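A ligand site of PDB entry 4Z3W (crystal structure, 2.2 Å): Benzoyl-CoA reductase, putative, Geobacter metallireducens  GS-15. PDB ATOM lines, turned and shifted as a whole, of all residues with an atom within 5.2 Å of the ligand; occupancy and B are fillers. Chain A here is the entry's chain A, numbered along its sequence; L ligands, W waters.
An oxygen (O3) of the ligand is in hydrogen-bond range of the side-chain hydroxyl (OG) of Ser 439. O1 of the ligand sits at hydrogen-bond distance from N of Ser 439, at 3.2 Å. OG of Ser 504 is in hydrogen-bond range of N4 of the ligand, 2.8 Å away. The backbone NH (N) of Met 440 lies within hydrogen-bond range of an oxygen (O1) of the ligand. The backbone carbonyl oxygen of Met 505 is in hydrogen-bond range of a nitrogen (N4) of the ligand (2.9 Å). The side-chain amide oxygen of Gln 466 is in hydrogen-bond range of a nitrogen (N6) of the ligand, 2.9 Å away. An oxygen (O2) of the ligand is in salt-bridge range of the guanidinium group of Arg 272 (3.8 Å). O7 of the ligand sits at hydrogen-bond distance from NH2 of Arg 500, at 2.9 Å.
N of Phe 323 sits close to OE1 of Glu 251 (3.3 Å). OH of Tyr 445 sits at hydrogen-bond distance from OE1 of Glu 461, 2.7 Å away. The backbone carbonyl oxygen of Trp 259 lies close to the side-chain amide oxygen of Asn 263, at 3.0 Å. OG of Ser 504 sits at hydrogen-bond distance from O of Gly 501. The guanidinium group of Arg 272 sits close to the side-chain amide nitrogen of Asn 263 (3.3 Å). A ring nitrogen (ND1) of His 260 lies within hydrogen-bond range of the side-chain carboxylate of Glu 251 (3.4 Å). The backbone carbonyl oxygen (O) of Ser 439 lies within hydrogen-bond range of the backbone NH (N) of Asn 602, 2.8 Å away. The backbone NH of Tyr 445 lies within hydrogen-bond range of the side-chain amide oxygen of Asn 442 (3.1 Å).
The side-chain carboxylate (OE2) of Glu 461 lies close to an oxygen (O8) of the ligand (2.9 Å). CG of Pro 249 touches C18 of the ligand (3.5 Å). Glu 251 touches the ligand (OE1 to C13, 3.9 Å). NE1 of Trp 259 touches C27 of the ligand, 3.4 Å away. His 260 touches the ligand (NE2 to C13, 3.2 Å). CZ of Phe 264 touches S1 of the ligand, at 3.9 Å. CG of Phe 323 touches C11 of the ligand (3.6 Å). Leu 434 touches the ligand. CD1 of Leu 436 touches O11 of the ligand, 3.3 Å away. Leu 438 touches the ligand (CD1 to O11, 3.6 Å). Tyr 445 touches the ligand. Ile 457 touches the ligand. Thr 458 touches the ligand. O of Pro 499 touches N4 of the ligand (3.8 Å). Hydrophobic or aromatic side chains within 4 Å of the ligand: Pro 249, Trp 259, His 260, Phe 264, Phe 323, Leu 434, Leu 436, Leu 438, Met 440, Tyr 445 and Ile 457. Of the 30 residues printed, 21 come within 4 Å of the ligand.
Water W1 lies within hydrogen-bond range of a nitrogen (N1) of the ligand, the backbone NH of Gly 501 and the side-chain hydroxyl of Ser 504. Water W2 lies within hydrogen-bond range of OH of Tyr 449 (2.5 Å) and O11 of the ligand (3.0 Å).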
ATOM      1  N   LEU A 243      -7.188  15.367 -15.776  1.00  0.00           N
ATOM      2  CA  LEU A 243      -7.817  14.093 -15.443  1.00  0.00           C
ATOM      3  C   LEU A 243      -6.898  12.909 -15.699  1.00  0.00           C
ATOM      4  O   LEU A 243      -7.366  11.793 -15.935  1.00  0.00           O
ATOM      5  CB  LEU A 243      -9.109  13.934 -16.246  1.00  0.00           C
ATOM      6  CG  LEU A 243     -10.114  15.072 -16.050  1.00  0.00           C
ATOM      7  CD1 LEU A 243     -11.201  15.044 -17.113  1.00  0.00           C
ATOM      8  CD2 LEU A 243     -10.711  15.025 -14.651  1.00  0.00           C
ATOM      9  N   PRO A 249     -10.483  17.260  -9.888  1.00  0.00           N
ATOM     10  CA  PRO A 249      -9.956  17.864 -11.127  1.00  0.00           C
ATOM     11  C   PRO A 249      -8.956  18.971 -10.816  1.00  0.00           C
ATOM     12  O   PRO A 249      -9.274  19.942 -10.150  1.00  0.00           O
ATOM     13  CB  PRO A 249     -11.220  18.413 -11.798  1.00  0.00           C
ATOM     14  CG  PRO A 249     -12.267  17.409 -11.392  1.00  0.00           C
ATOM     15  CD  PRO A 249     -11.924  16.982  -9.976  1.00  0.00           C
ATOM     16  N   GLU A 251      -7.656  21.651 -11.548  1.00  0.00           N
ATOM     17  CA  GLU A 251      -7.755  22.895 -12.299  1.00  0.00           C
ATOM     18  C   GLU A 251      -7.036  24.082 -11.686  1.00  0.00           C
ATOM     19  O   GLU A 251      -6.826  25.088 -12.369  1.00  0.00           O
ATOM     20  CB  GLU A 251      -9.219  23.240 -12.513  1.00  0.00           C
ATOM     21  CG  GLU A 251      -9.856  22.450 -13.663  1.00  0.00           C
ATOM     22  CD  GLU A 251     -11.289  22.793 -13.789  1.00  0.00           C
ATOM     23  OE1 GLU A 251     -12.111  22.128 -13.116  1.00  0.00           O
ATOM     24  OE2 GLU A 251     -11.596  23.746 -14.514  1.00  0.00           O
ATOM     25  N   TRP A 259     -10.186  21.559 -23.142  1.00  0.00           N
ATOM     26  CA  TRP A 259     -11.221  20.552 -23.082  1.00  0.00           C
ATOM     27  C   TRP A 259     -12.518  21.177 -22.613  1.00  0.00           C
ATOM     28  O   TRP A 259     -13.546  21.071 -23.282  1.00  0.00           O
ATOM     29  CB  TRP A 259     -10.801  19.396 -22.177  1.00  0.00           C
ATOM     30  CG  TRP A 259     -11.837  18.323 -22.029  1.00  0.00           C
ATOM     31  CD1 TRP A 259     -12.299  17.484 -23.006  1.00  0.00           C
ATOM     32  CD2 TRP A 259     -12.536  17.962 -20.823  1.00  0.00           C
ATOM     33  NE1 TRP A 259     -13.253  16.636 -22.489  1.00  0.00           N
ATOM     34  CE2 TRP A 259     -13.414  16.913 -21.155  1.00  0.00           C
ATOM     35  CE3 TRP A 259     -12.517  18.426 -19.503  1.00  0.00           C
ATOM     36  CZ2 TRP A 259     -14.252  16.306 -20.212  1.00  0.00           C
ATOM     37  CZ3 TRP A 259     -13.350  17.831 -18.571  1.00  0.00           C
ATOM     38  CH2 TRP A 259     -14.207  16.776 -18.924  1.00  0.00           C
ATOM     39  N   HIS A 260     -12.469  21.848 -21.459  1.00  0.00           N
ATOM     40  CA  HIS A 260     -13.622  22.522 -20.874  1.00  0.00           C
ATOM     41  C   HIS A 260     -14.233  23.627 -21.741  1.00  0.00           C
ATOM     42  O   HIS A 260     -15.448  23.663 -21.943  1.00  0.00           O
ATOM     43  CB  HIS A 260     -13.245  23.136 -19.536  1.00  0.00           C
ATOM     44  CG  HIS A 260     -13.325  22.192 -18.381  1.00  0.00           C
ATOM     45  ND1 HIS A 260     -12.394  22.162 -17.372  1.00  0.00           N
ATOM     46  CD2 HIS A 260     -14.247  21.252 -18.067  1.00  0.00           C
ATOM     47  CE1 HIS A 260     -12.727  21.238 -16.489  1.00  0.00           C
ATOM     48  NE2 HIS A 260     -13.855  20.671 -16.880  1.00  0.00           N
ATOM     49  N   ASN A 263     -15.634  22.319 -25.314  1.00  0.00           N
ATOM     50  CA  ASN A 263     -16.603  21.224 -25.353  1.00  0.00           C
ATOM     51  C   ASN A 263     -17.807  21.425 -24.452  1.00  0.00           C
ATOM     52  O   ASN A 263     -18.844  20.817 -24.669  1.00  0.00           O
ATOM     53  CB  ASN A 263     -15.914  19.902 -24.984  1.00  0.00           C
ATOM     54  CG  ASN A 263     -14.896  19.472 -26.025  1.00  0.00           C
ATOM     55  OD1 ASN A 263     -13.719  19.279 -25.705  1.00  0.00           O
ATOM     56  ND2 ASN A 263     -15.336  19.335 -27.262  1.00  0.00           N
ATOM     57  N   PHE A 264     -17.662  22.260 -23.417  1.00  0.00           N
ATOM     58  CA  PHE A 264     -18.783  22.613 -22.558  1.00  0.00           C
ATOM     59  C   PHE A 264     -19.487  23.874 -23.071  1.00  0.00           C
ATOM     60  O   PHE A 264     -18.875  24.703 -23.709  1.00  0.00           O
ATOM     61  CB  PHE A 264     -18.306  22.821 -21.117  1.00  0.00           C
ATOM     62  CG  PHE A 264     -17.894  21.556 -20.407  1.00  0.00           C
ATOM     63  CD1 PHE A 264     -16.907  20.737 -20.948  1.00  0.00           C
ATOM     64  CD2 PHE A 264     -18.480  21.184 -19.201  1.00  0.00           C
ATOM     65  CE1 PHE A 264     -16.522  19.578 -20.293  1.00  0.00           C
ATOM     66  CE2 PHE A 264     -18.101  20.029 -18.552  1.00  0.00           C
ATOM     67  CZ  PHE A 264     -17.122  19.225 -19.091  1.00  0.00           C
ATOM     68  N   ARG A 272     -21.911  26.408 -27.740  1.00  0.00           N
ATOM     69  CA  ARG A 272     -20.625  25.759 -27.939  1.00  0.00           C
ATOM     70  C   ARG A 272     -19.694  26.708 -28.692  1.00  0.00           C
ATOM     71  O   ARG A 272     -20.115  27.402 -29.622  1.00  0.00           O
ATOM     72  CB  ARG A 272     -20.756  24.439 -28.692  1.00  0.00           C
ATOM     73  CG  ARG A 272     -19.488  23.572 -28.610  1.00  0.00           C
ATOM     74  CD  ARG A 272     -19.704  22.190 -29.215  1.00  0.00           C
ATOM     75  NE  ARG A 272     -18.952  21.166 -28.501  1.00  0.00           N
ATOM     76  CZ  ARG A 272     -19.281  19.880 -28.454  1.00  0.00           C
ATOM     77  NH1 ARG A 272     -20.363  19.442 -29.105  1.00  0.00           N
ATOM     78  NH2 ARG A 272     -18.532  19.025 -27.773  1.00  0.00           N
ATOM     79  N   CYS A 322     -11.454  22.811  -8.342  1.00  0.00           N
ATOM     80  CA  CYS A 322     -12.320  22.240  -9.361  1.00  0.00           C
ATOM     81  C   CYS A 322     -13.040  23.285 -10.234  1.00  0.00           C
ATOM     82  O   CYS A 322     -12.531  24.378 -10.468  1.00  0.00           O
ATOM     83  CB  CYS A 322     -13.344  21.311  -8.692  1.00  0.00           C
ATOM     84  SG  CYS A 322     -14.070  20.038  -9.791  1.00  0.00           S
ATOM     85  N   PHE A 323     -14.252  22.948 -10.696  1.00  0.00           N
ATOM     86  CA  PHE A 323     -14.836  23.587 -11.875  1.00  0.00           C
ATOM     87  C   PHE A 323     -15.471  24.960 -11.615  1.00  0.00           C
ATOM     88  O   PHE A 323     -15.824  25.680 -12.555  1.00  0.00           O
ATOM     89  CB  PHE A 323     -15.864  22.621 -12.479  1.00  0.00           C
ATOM     90  CG  PHE A 323     -16.361  22.992 -13.861  1.00  0.00           C
ATOM     91  CD1 PHE A 323     -15.505  23.523 -14.810  1.00  0.00           C
ATOM     92  CD2 PHE A 323     -17.686  22.745 -14.229  1.00  0.00           C
ATOM     93  CE1 PHE A 323     -15.961  23.847 -16.082  1.00  0.00           C
ATOM     94  CE2 PHE A 323     -18.148  23.041 -15.514  1.00  0.00           C
ATOM     95  CZ  PHE A 323     -17.291  23.589 -16.438  1.00  0.00           C
ATOM     96  N   LEU A 434     -24.581  19.694 -15.354  1.00  0.00           N
ATOM     97  CA  LEU A 434     -23.424  20.302 -16.008  1.00  0.00           C
ATOM     98  C   LEU A 434     -23.775  20.777 -17.415  1.00  0.00           C
ATOM     99  O   LEU A 434     -24.572  20.151 -18.106  1.00  0.00           O
ATOM    100  CB  LEU A 434     -22.277  19.321 -16.060  1.00  0.00           C
ATOM    101  CG  LEU A 434     -21.516  19.276 -14.729  1.00  0.00           C
ATOM    102  CD1 LEU A 434     -20.582  18.104 -14.729  1.00  0.00           C
ATOM    103  CD2 LEU A 434     -20.729  20.558 -14.562  1.00  0.00           C
ATOM    104  N   LEU A 436     -23.350  20.535 -20.547  1.00  0.00           N
ATOM    105  CA  LEU A 436     -22.903  19.684 -21.649  1.00  0.00           C
ATOM    106  C   LEU A 436     -24.045  19.385 -22.611  1.00  0.00           C
ATOM    107  O   LEU A 436     -25.043  18.753 -22.236  1.00  0.00           O
ATOM    108  CB  LEU A 436     -22.338  18.380 -21.092  1.00  0.00           C
ATOM    109  CG  LEU A 436     -20.938  18.363 -20.494  1.00  0.00           C
ATOM    110  CD1 LEU A 436     -20.906  17.406 -19.325  1.00  0.00           C
ATOM    111  CD2 LEU A 436     -19.935  17.933 -21.551  1.00  0.00           C
ATOM    112  N   LEU A 438     -23.904  17.506 -25.949  1.00  0.00           N
ATOM    113  CA  LEU A 438     -23.044  16.772 -26.868  1.00  0.00           C
ATOM    114  C   LEU A 438     -23.838  16.270 -28.091  1.00  0.00           C
ATOM    115  O   LEU A 438     -25.044  16.482 -28.186  1.00  0.00           O
ATOM    116  CB  LEU A 438     -22.364  15.616 -26.121  1.00  0.00           C
ATOM    117  CG  LEU A 438     -21.538  16.070 -24.911  1.00  0.00           C
ATOM    118  CD1 LEU A 438     -20.836  14.898 -24.237  1.00  0.00           C
ATOM    119  CD2 LEU A 438     -20.519  17.129 -25.345  1.00  0.00           C
ATOM    120  N   SER A 439     -23.141  15.620 -29.023  1.00  0.00           N
ATOM    121  CA  SER A 439     -23.785  15.248 -30.288  1.00  0.00           C
ATOM    122  C   SER A 439     -24.382  13.837 -30.260  1.00  0.00           C
ATOM    123  O   SER A 439     -25.550  13.651 -30.588  1.00  0.00           O
ATOM    124  CB  SER A 439     -22.788  15.380 -31.439  1.00  0.00           C
ATOM    125  OG  SER A 439     -23.392  15.025 -32.667  1.00  0.00           O
ATOM    126  N   MET A 440     -23.587  12.855 -29.859  1.00  0.00           N
ATOM    127  CA  MET A 440     -23.993  11.448 -29.915  1.00  0.00           C
ATOM    128  C   MET A 440     -24.369  10.876 -28.548  1.00  0.00           C
ATOM    129  O   MET A 440     -23.650  11.055 -27.589  1.00  0.00           O
ATOM    130  CB  MET A 440     -22.865  10.611 -30.527  1.00  0.00           C
ATOM    131  CG  MET A 440     -23.225   9.141 -30.750  1.00  0.00           C
ATOM    132  SD  MET A 440     -24.587   8.910 -31.921  1.00  0.00           S
ATOM    133  CE  MET A 440     -23.794   9.451 -33.452  1.00  0.00           C
ATOM    134  N   ASN A 442     -24.574   8.839 -25.368  1.00  0.00           N
ATOM    135  CA  ASN A 442     -23.593   8.053 -24.645  1.00  0.00           C
ATOM    136  C   ASN A 442     -24.356   7.152 -23.680  1.00  0.00           C
ATOM    137  O   ASN A 442     -24.864   7.609 -22.668  1.00  0.00           O
ATOM    138  CB  ASN A 442     -22.609   8.961 -23.897  1.00  0.00           C
ATOM    139  CG  ASN A 442     -21.467   8.198 -23.221  1.00  0.00           C
ATOM    140  OD1 ASN A 442     -21.716   7.191 -22.549  1.00  0.00           O
ATOM    141  ND2 ASN A 442     -20.229   8.676 -23.402  1.00  0.00           N
ATOM    142  N   TYR A 445     -23.350   7.312 -19.930  1.00  0.00           N
ATOM    143  CA  TYR A 445     -23.687   8.580 -19.274  1.00  0.00           C
ATOM    144  C   TYR A 445     -25.187   8.770 -19.196  1.00  0.00           C
ATOM    145  O   TYR A 445     -25.698   9.380 -18.241  1.00  0.00           O
ATOM    146  CB  TYR A 445     -23.007   9.756 -19.976  1.00  0.00           C
ATOM    147  CG  TYR A 445     -21.599   9.914 -19.458  1.00  0.00           C
ATOM    148  CD1 TYR A 445     -20.587   9.047 -19.848  1.00  0.00           C
ATOM    149  CD2 TYR A 445     -21.298  10.905 -18.538  1.00  0.00           C
ATOM    150  CE1 TYR A 445     -19.314   9.188 -19.360  1.00  0.00           C
ATOM    151  CE2 TYR A 445     -20.037  11.036 -18.032  1.00  0.00           C
ATOM    152  CZ  TYR A 445     -19.037  10.178 -18.435  1.00  0.00           C
ATOM    153  OH  TYR A 445     -17.772  10.318 -17.927  1.00  0.00           O
ATOM    154  N   TYR A 449     -26.993   9.931 -15.741  1.00  0.00           N
ATOM    155  CA  TYR A 449     -27.873  11.084 -15.624  1.00  0.00           C
ATOM    156  C   TYR A 449     -29.252  10.666 -15.068  1.00  0.00           C
ATOM    157  O   TYR A 449     -29.781  11.305 -14.153  1.00  0.00           O
ATOM    158  CB  TYR A 449     -28.061  11.775 -16.982  1.00  0.00           C
ATOM    159  CG  TYR A 449     -26.898  12.616 -17.431  1.00  0.00           C
ATOM    160  CD1 TYR A 449     -26.486  13.722 -16.703  1.00  0.00           C
ATOM    161  CD2 TYR A 449     -26.224  12.321 -18.607  1.00  0.00           C
ATOM    162  CE1 TYR A 449     -25.406  14.506 -17.120  1.00  0.00           C
ATOM    163  CE2 TYR A 449     -25.140  13.081 -19.028  1.00  0.00           C
ATOM    164  CZ  TYR A 449     -24.741  14.178 -18.281  1.00  0.00           C
ATOM    165  OH  TYR A 449     -23.685  14.944 -18.719  1.00  0.00           O
ATOM    166  N   ILE A 457     -23.555  14.510 -12.516  1.00  0.00           N
ATOM    167  CA  ILE A 457     -22.725  13.600 -13.305  1.00  0.00           C
ATOM    168  C   ILE A 457     -21.284  13.507 -12.761  1.00  0.00           C
ATOM    169  O   ILE A 457     -20.676  12.441 -12.813  1.00  0.00           O
ATOM    170  CB  ILE A 457     -22.713  14.029 -14.797  1.00  0.00           C
ATOM    171  CG1 ILE A 457     -22.422  12.830 -15.691  1.00  0.00           C
ATOM    172  CG2 ILE A 457     -21.734  15.163 -15.032  1.00  0.00           C
ATOM    173  CD1 ILE A 457     -23.429  11.721 -15.547  1.00  0.00           C
ATOM    174  N   THR A 458     -20.723  14.597 -12.225  1.00  0.00           N
ATOM    175  CA  THR A 458     -19.309  14.499 -11.794  1.00  0.00           C
ATOM    176  C   THR A 458     -19.187  13.738 -10.484  1.00  0.00           C
ATOM    177  O   THR A 458     -18.085  13.487 -10.008  1.00  0.00           O
ATOM    178  CB  THR A 458     -18.625  15.877 -11.625  1.00  0.00           C
ATOM    179  OG1 THR A 458     -19.248  16.609 -10.569  1.00  0.00           O
ATOM    180  CG2 THR A 458     -18.679  16.677 -12.906  1.00  0.00           C
ATOM    181  N   GLU A 461     -19.532   9.372 -11.955  1.00  0.00           N
ATOM    182  CA  GLU A 461     -18.547   8.857 -12.907  1.00  0.00           C
ATOM    183  C   GLU A 461     -17.183   8.606 -12.256  1.00  0.00           C
ATOM    184  O   GLU A 461     -16.978   8.922 -11.085  1.00  0.00           O
ATOM    185  CB  GLU A 461     -18.359   9.856 -14.041  1.00  0.00           C
ATOM    186  CG  GLU A 461     -17.380  10.967 -13.652  1.00  0.00           C
ATOM    187  CD  GLU A 461     -17.360  12.119 -14.649  1.00  0.00           C
ATOM    188  OE1 GLU A 461     -17.862  11.953 -15.781  1.00  0.00           O
ATOM    189  OE2 GLU A 461     -16.836  13.188 -14.286  1.00  0.00           O
ATOM    190  N   GLN A 466     -13.550   7.846 -19.867  1.00  0.00           N
ATOM    191  CA  GLN A 466     -14.619   8.566 -20.560  1.00  0.00           C
ATOM    192  C   GLN A 466     -14.630   8.327 -22.075  1.00  0.00           C
ATOM    193  O   GLN A 466     -15.638   8.564 -22.741  1.00  0.00           O
ATOM    194  CB  GLN A 466     -14.510  10.073 -20.309  1.00  0.00           C
ATOM    195  CG  GLN A 466     -14.745  10.500 -18.873  1.00  0.00           C
ATOM    196  CD  GLN A 466     -15.000  11.990 -18.751  1.00  0.00           C
ATOM    197  OE1 GLN A 466     -15.417  12.643 -19.710  1.00  0.00           O
ATOM    198  NE2 GLN A 466     -14.763  12.546 -17.553  1.00  0.00           N
ATOM    199  N   PRO A 499     -13.085   4.153 -30.701  1.00  0.00           N
ATOM    200  CA  PRO A 499     -13.642   5.471 -30.994  1.00  0.00           C
ATOM    201  C   PRO A 499     -14.607   5.466 -32.172  1.00  0.00           C
ATOM    202  O   PRO A 499     -15.605   6.206 -32.139  1.00  0.00           O
ATOM    203  CB  PRO A 499     -12.407   6.327 -31.318  1.00  0.00           C
ATOM    204  CG  PRO A 499     -11.311   5.372 -31.514  1.00  0.00           C
ATOM    205  CD  PRO A 499     -11.613   4.146 -30.723  1.00  0.00           C
ATOM    206  N   ARG A 500     -14.328   4.644 -33.189  1.00  0.00           N
ATOM    207  CA  ARG A 500     -15.117   4.630 -34.404  1.00  0.00           C
ATOM    208  C   ARG A 500     -15.314   3.222 -34.940  1.00  0.00           C
ATOM    209  O   ARG A 500     -14.438   2.375 -34.795  1.00  0.00           O
ATOM    210  CB  ARG A 500     -14.442   5.498 -35.477  1.00  0.00           C
ATOM    211  CG  ARG A 500     -14.448   6.994 -35.180  1.00  0.00           C
ATOM    212  CD  ARG A 500     -15.844   7.571 -35.358  1.00  0.00           C
ATOM    213  NE  ARG A 500     -15.837   9.034 -35.327  1.00  0.00           N
ATOM    214  CZ  ARG A 500     -15.990   9.775 -34.235  1.00  0.00           C
ATOM    215  NH1 ARG A 500     -16.164   9.200 -33.039  1.00  0.00           N
ATOM    216  NH2 ARG A 500     -15.967  11.098 -34.324  1.00  0.00           N
ATOM    217  N   GLY A 501     -16.464   2.981 -35.552  1.00  0.00           N
ATOM    218  CA  GLY A 501     -16.715   1.705 -36.190  1.00  0.00           C
ATOM    219  C   GLY A 501     -17.685   0.850 -35.416  1.00  0.00           C
ATOM    220  O   GLY A 501     -18.407   1.355 -34.543  1.00  0.00           O
ATOM    221  N   SER A 504     -18.067   0.992 -31.525  1.00  0.00           N
ATOM    222  CA  SER A 504     -18.152   2.325 -30.949  1.00  0.00           C
ATOM    223  C   SER A 504     -19.556   2.622 -30.416  1.00  0.00           C
ATOM    224  O   SER A 504     -20.496   1.860 -30.669  1.00  0.00           O
ATOM    225  CB  SER A 504     -17.743   3.374 -31.989  1.00  0.00           C
ATOM    226  OG  SER A 504     -18.730   3.531 -32.986  1.00  0.00           O
ATOM    227  N   MET A 505     -19.697   3.712 -29.660  1.00  0.00           N
ATOM    228  CA  MET A 505     -21.007   4.133 -29.124  1.00  0.00           C
ATOM    229  C   MET A 505     -21.879   4.683 -30.237  1.00  0.00           C
ATOM    230  O   MET A 505     -21.365   5.211 -31.224  1.00  0.00           O
ATOM    231  CB  MET A 505     -20.828   5.195 -28.012  1.00  0.00           C
ATOM    232  CG  MET A 505     -20.246   4.663 -26.705  1.00  0.00           C
ATOM    233  SD  MET A 505     -19.956   5.945 -25.454  1.00  0.00           S
ATOM    234  CE  MET A 505     -19.783   4.935 -23.972  1.00  0.00           C
ATOM    235  N   PRO A 506     -23.208   4.611 -30.080  1.00  0.00           N
ATOM    236  CA  PRO A 506     -23.929   4.222 -28.860  1.00  0.00           C
ATOM    237  C   PRO A 506     -24.161   2.716 -28.717  1.00  0.00           C
ATOM    238  O   PRO A 506     -24.626   2.273 -27.658  1.00  0.00           O
ATOM    239  CB  PRO A 506     -25.261   4.944 -29.012  1.00  0.00           C
ATOM    240  CG  PRO A 506     -25.499   4.932 -30.481  1.00  0.00           C
ATOM    241  CD  PRO A 506     -24.144   4.969 -31.163  1.00  0.00           C
ATOM    242  N   PHE A 540     -13.158   8.910  -8.130  1.00  0.00           N
ATOM    243  CA  PHE A 540     -13.166   9.882  -9.222  1.00  0.00           C
ATOM    244  C   PHE A 540     -12.097   9.618 -10.299  1.00  0.00           C
ATOM    245  O   PHE A 540     -12.425   9.562 -11.489  1.00  0.00           O
ATOM    246  CB  PHE A 540     -13.041  11.304  -8.690  1.00  0.00           C
ATOM    247  CG  PHE A 540     -13.192  12.352  -9.758  1.00  0.00           C
ATOM    248  CD1 PHE A 540     -12.110  12.778 -10.497  1.00  0.00           C
ATOM    249  CD2 PHE A 540     -14.443  12.890 -10.025  1.00  0.00           C
ATOM    250  CE1 PHE A 540     -12.256  13.740 -11.495  1.00  0.00           C
ATOM    251  CE2 PHE A 540     -14.605  13.836 -11.020  1.00  0.00           C
ATOM    252  CZ  PHE A 540     -13.506  14.264 -11.757  1.00  0.00           C
ATOM    253  N   ASN A 602     -28.303  13.374 -31.154  1.00  0.00           N
ATOM    254  CA  ASN A 602     -28.696  12.065 -31.695  1.00  0.00           C
ATOM    255  C   ASN A 602     -29.270  11.177 -30.603  1.00  0.00           C
ATOM    256  O   ASN A 602     -28.547  10.713 -29.732  1.00  0.00           O
ATOM    257  CB  ASN A 602     -27.505  11.357 -32.363  1.00  0.00           C
ATOM    258  CG  ASN A 602     -27.025  12.057 -33.616  1.00  0.00           C
ATOM    259  OD1 ASN A 602     -26.706  13.242 -33.604  1.00  0.00           O
ATOM    260  ND2 ASN A 602     -26.972  11.320 -34.709  1.00  0.00           N
HETATM  261  N1  LIG L   1     -19.186   7.179 -35.073  1.00  0.00           N
HETATM  262  O1  LIG L   1     -20.847  13.434 -28.997  1.00  0.00           O
HETATM  263  P1  LIG L   1     -19.666  14.263 -29.484  1.00  0.00           P
HETATM  264  C1  LIG L   1     -16.749  16.112 -16.148  1.00  0.00           C
HETATM  265  C2  LIG L   1     -19.514  12.199 -33.984  1.00  0.00           C
HETATM  266  S1  LIG L   1     -18.394  16.449 -16.670  1.00  0.00           S
HETATM  267  C3  LIG L   1     -19.175   8.263 -35.860  1.00  0.00           C
HETATM  268  O2  LIG L   1     -19.954  15.721 -29.487  1.00  0.00           O
HETATM  269  P2  LIG L   1     -16.962  14.448 -28.427  1.00  0.00           P
HETATM  270  C4  LIG L   1     -16.090  17.224 -15.433  1.00  0.00           C
HETATM  271  C5  LIG L   1     -20.608  13.122 -33.462  1.00  0.00           C
HETATM  272  O3  LIG L   1     -21.783  13.087 -34.267  1.00  0.00           O
HETATM  273  C6  LIG L   1     -18.777  15.008 -17.728  1.00  0.00           C
HETATM  274  N2  LIG L   1     -19.319   9.543 -35.516  1.00  0.00           N
HETATM  275  O4  LIG L   1     -18.482  13.978 -28.458  1.00  0.00           O
HETATM  276  C7  LIG L   1     -16.759  18.466 -15.172  1.00  0.00           C
HETATM  277  C8  LIG L   1     -19.892  14.473 -33.584  1.00  0.00           C
HETATM  278  O5  LIG L   1     -19.934  14.996 -34.925  1.00  0.00           O
HETATM  279  P3  LIG L   1     -20.473  16.463 -35.354  1.00  0.00           P
HETATM  280  C9  LIG L   1     -17.856  14.893 -18.934  1.00  0.00           C
HETATM  281  C10 LIG L   1     -19.475   9.672 -34.196  1.00  0.00           C
HETATM  282  O6  LIG L   1     -16.710  15.576 -29.371  1.00  0.00           O
HETATM  283  C11 LIG L   1     -16.123  19.438 -14.544  1.00  0.00           C
HETATM  284  C12 LIG L   1     -18.456  14.131 -33.183  1.00  0.00           C
HETATM  285  O7  LIG L   1     -18.286  12.744 -33.560  1.00  0.00           O
HETATM  286  N3  LIG L   1     -18.161  13.699 -19.706  1.00  0.00           N
HETATM  287  O8  LIG L   1     -16.215  15.044 -16.373  1.00  0.00           O
HETATM  288  O9  LIG L   1     -16.109  13.195 -28.688  1.00  0.00           O
HETATM  289  C13 LIG L   1     -14.722  19.390 -14.053  1.00  0.00           C
HETATM  290  C14 LIG L   1     -18.141  14.300 -31.720  1.00  0.00           C
HETATM  291  O10 LIG L   1     -19.166  13.700 -30.893  1.00  0.00           O
HETATM  292  C15 LIG L   1     -19.518   8.647 -33.256  1.00  0.00           C
HETATM  293  C16 LIG L   1     -19.183  13.624 -20.563  1.00  0.00           C
HETATM  294  O11 LIG L   1     -19.939  14.571 -20.757  1.00  0.00           O
HETATM  295  C17 LIG L   1     -19.352   7.333 -33.742  1.00  0.00           C
HETATM  296  N4  LIG L   1     -19.352   6.256 -32.961  1.00  0.00           N
HETATM  297  O12 LIG L   1     -16.752  14.961 -26.942  1.00  0.00           O
HETATM  298  C18 LIG L   1     -13.985  18.095 -14.376  1.00  0.00           C
HETATM  299  C19 LIG L   1     -19.371  12.317 -21.303  1.00  0.00           C
HETATM  300  N5  LIG L   1     -19.676   9.153 -31.979  1.00  0.00           N
HETATM  301  O13 LIG L   1     -19.393  17.478 -35.256  1.00  0.00           O
HETATM  302  C20 LIG L   1     -14.824  17.050 -15.043  1.00  0.00           C
HETATM  303  C21 LIG L   1     -18.087  11.551 -21.489  1.00  0.00           C
HETATM  304  C22 LIG L   1     -19.726  10.455 -32.165  1.00  0.00           C
HETATM  305  O14 LIG L   1     -21.662  16.758 -34.448  1.00  0.00           O
HETATM  306  N6  LIG L   1     -17.065  12.381 -22.120  1.00  0.00           N
HETATM  307  N7  LIG L   1     -19.600  10.841 -33.474  1.00  0.00           N
HETATM  308  O15 LIG L   1     -21.011  16.306 -36.784  1.00  0.00           O
HETATM  309  C23 LIG L   1     -16.894  12.395 -23.447  1.00  0.00           C
HETATM  310  O16 LIG L   1     -17.627  11.803 -24.227  1.00  0.00           O
HETATM  311  C24 LIG L   1     -15.716  13.202 -23.974  1.00  0.00           C
HETATM  312  O17 LIG L   1     -14.795  13.500 -22.930  1.00  0.00           O
HETATM  313  C25 LIG L   1     -16.220  14.519 -24.616  1.00  0.00           C
HETATM  314  C26 LIG L   1     -17.093  14.145 -25.822  1.00  0.00           C
HETATM  315  C27 LIG L   1     -15.040  15.362 -25.107  1.00  0.00           C
HETATM  316  C28 LIG L   1     -17.057  15.315 -23.618  1.00  0.00           C
HETATM  317  O   HOH W   1     -18.511   4.751 -36.215  1.00  0.00           O
HETATM  318  O   HOH W   2     -22.917  14.203 -20.949  1.00  0.00           O
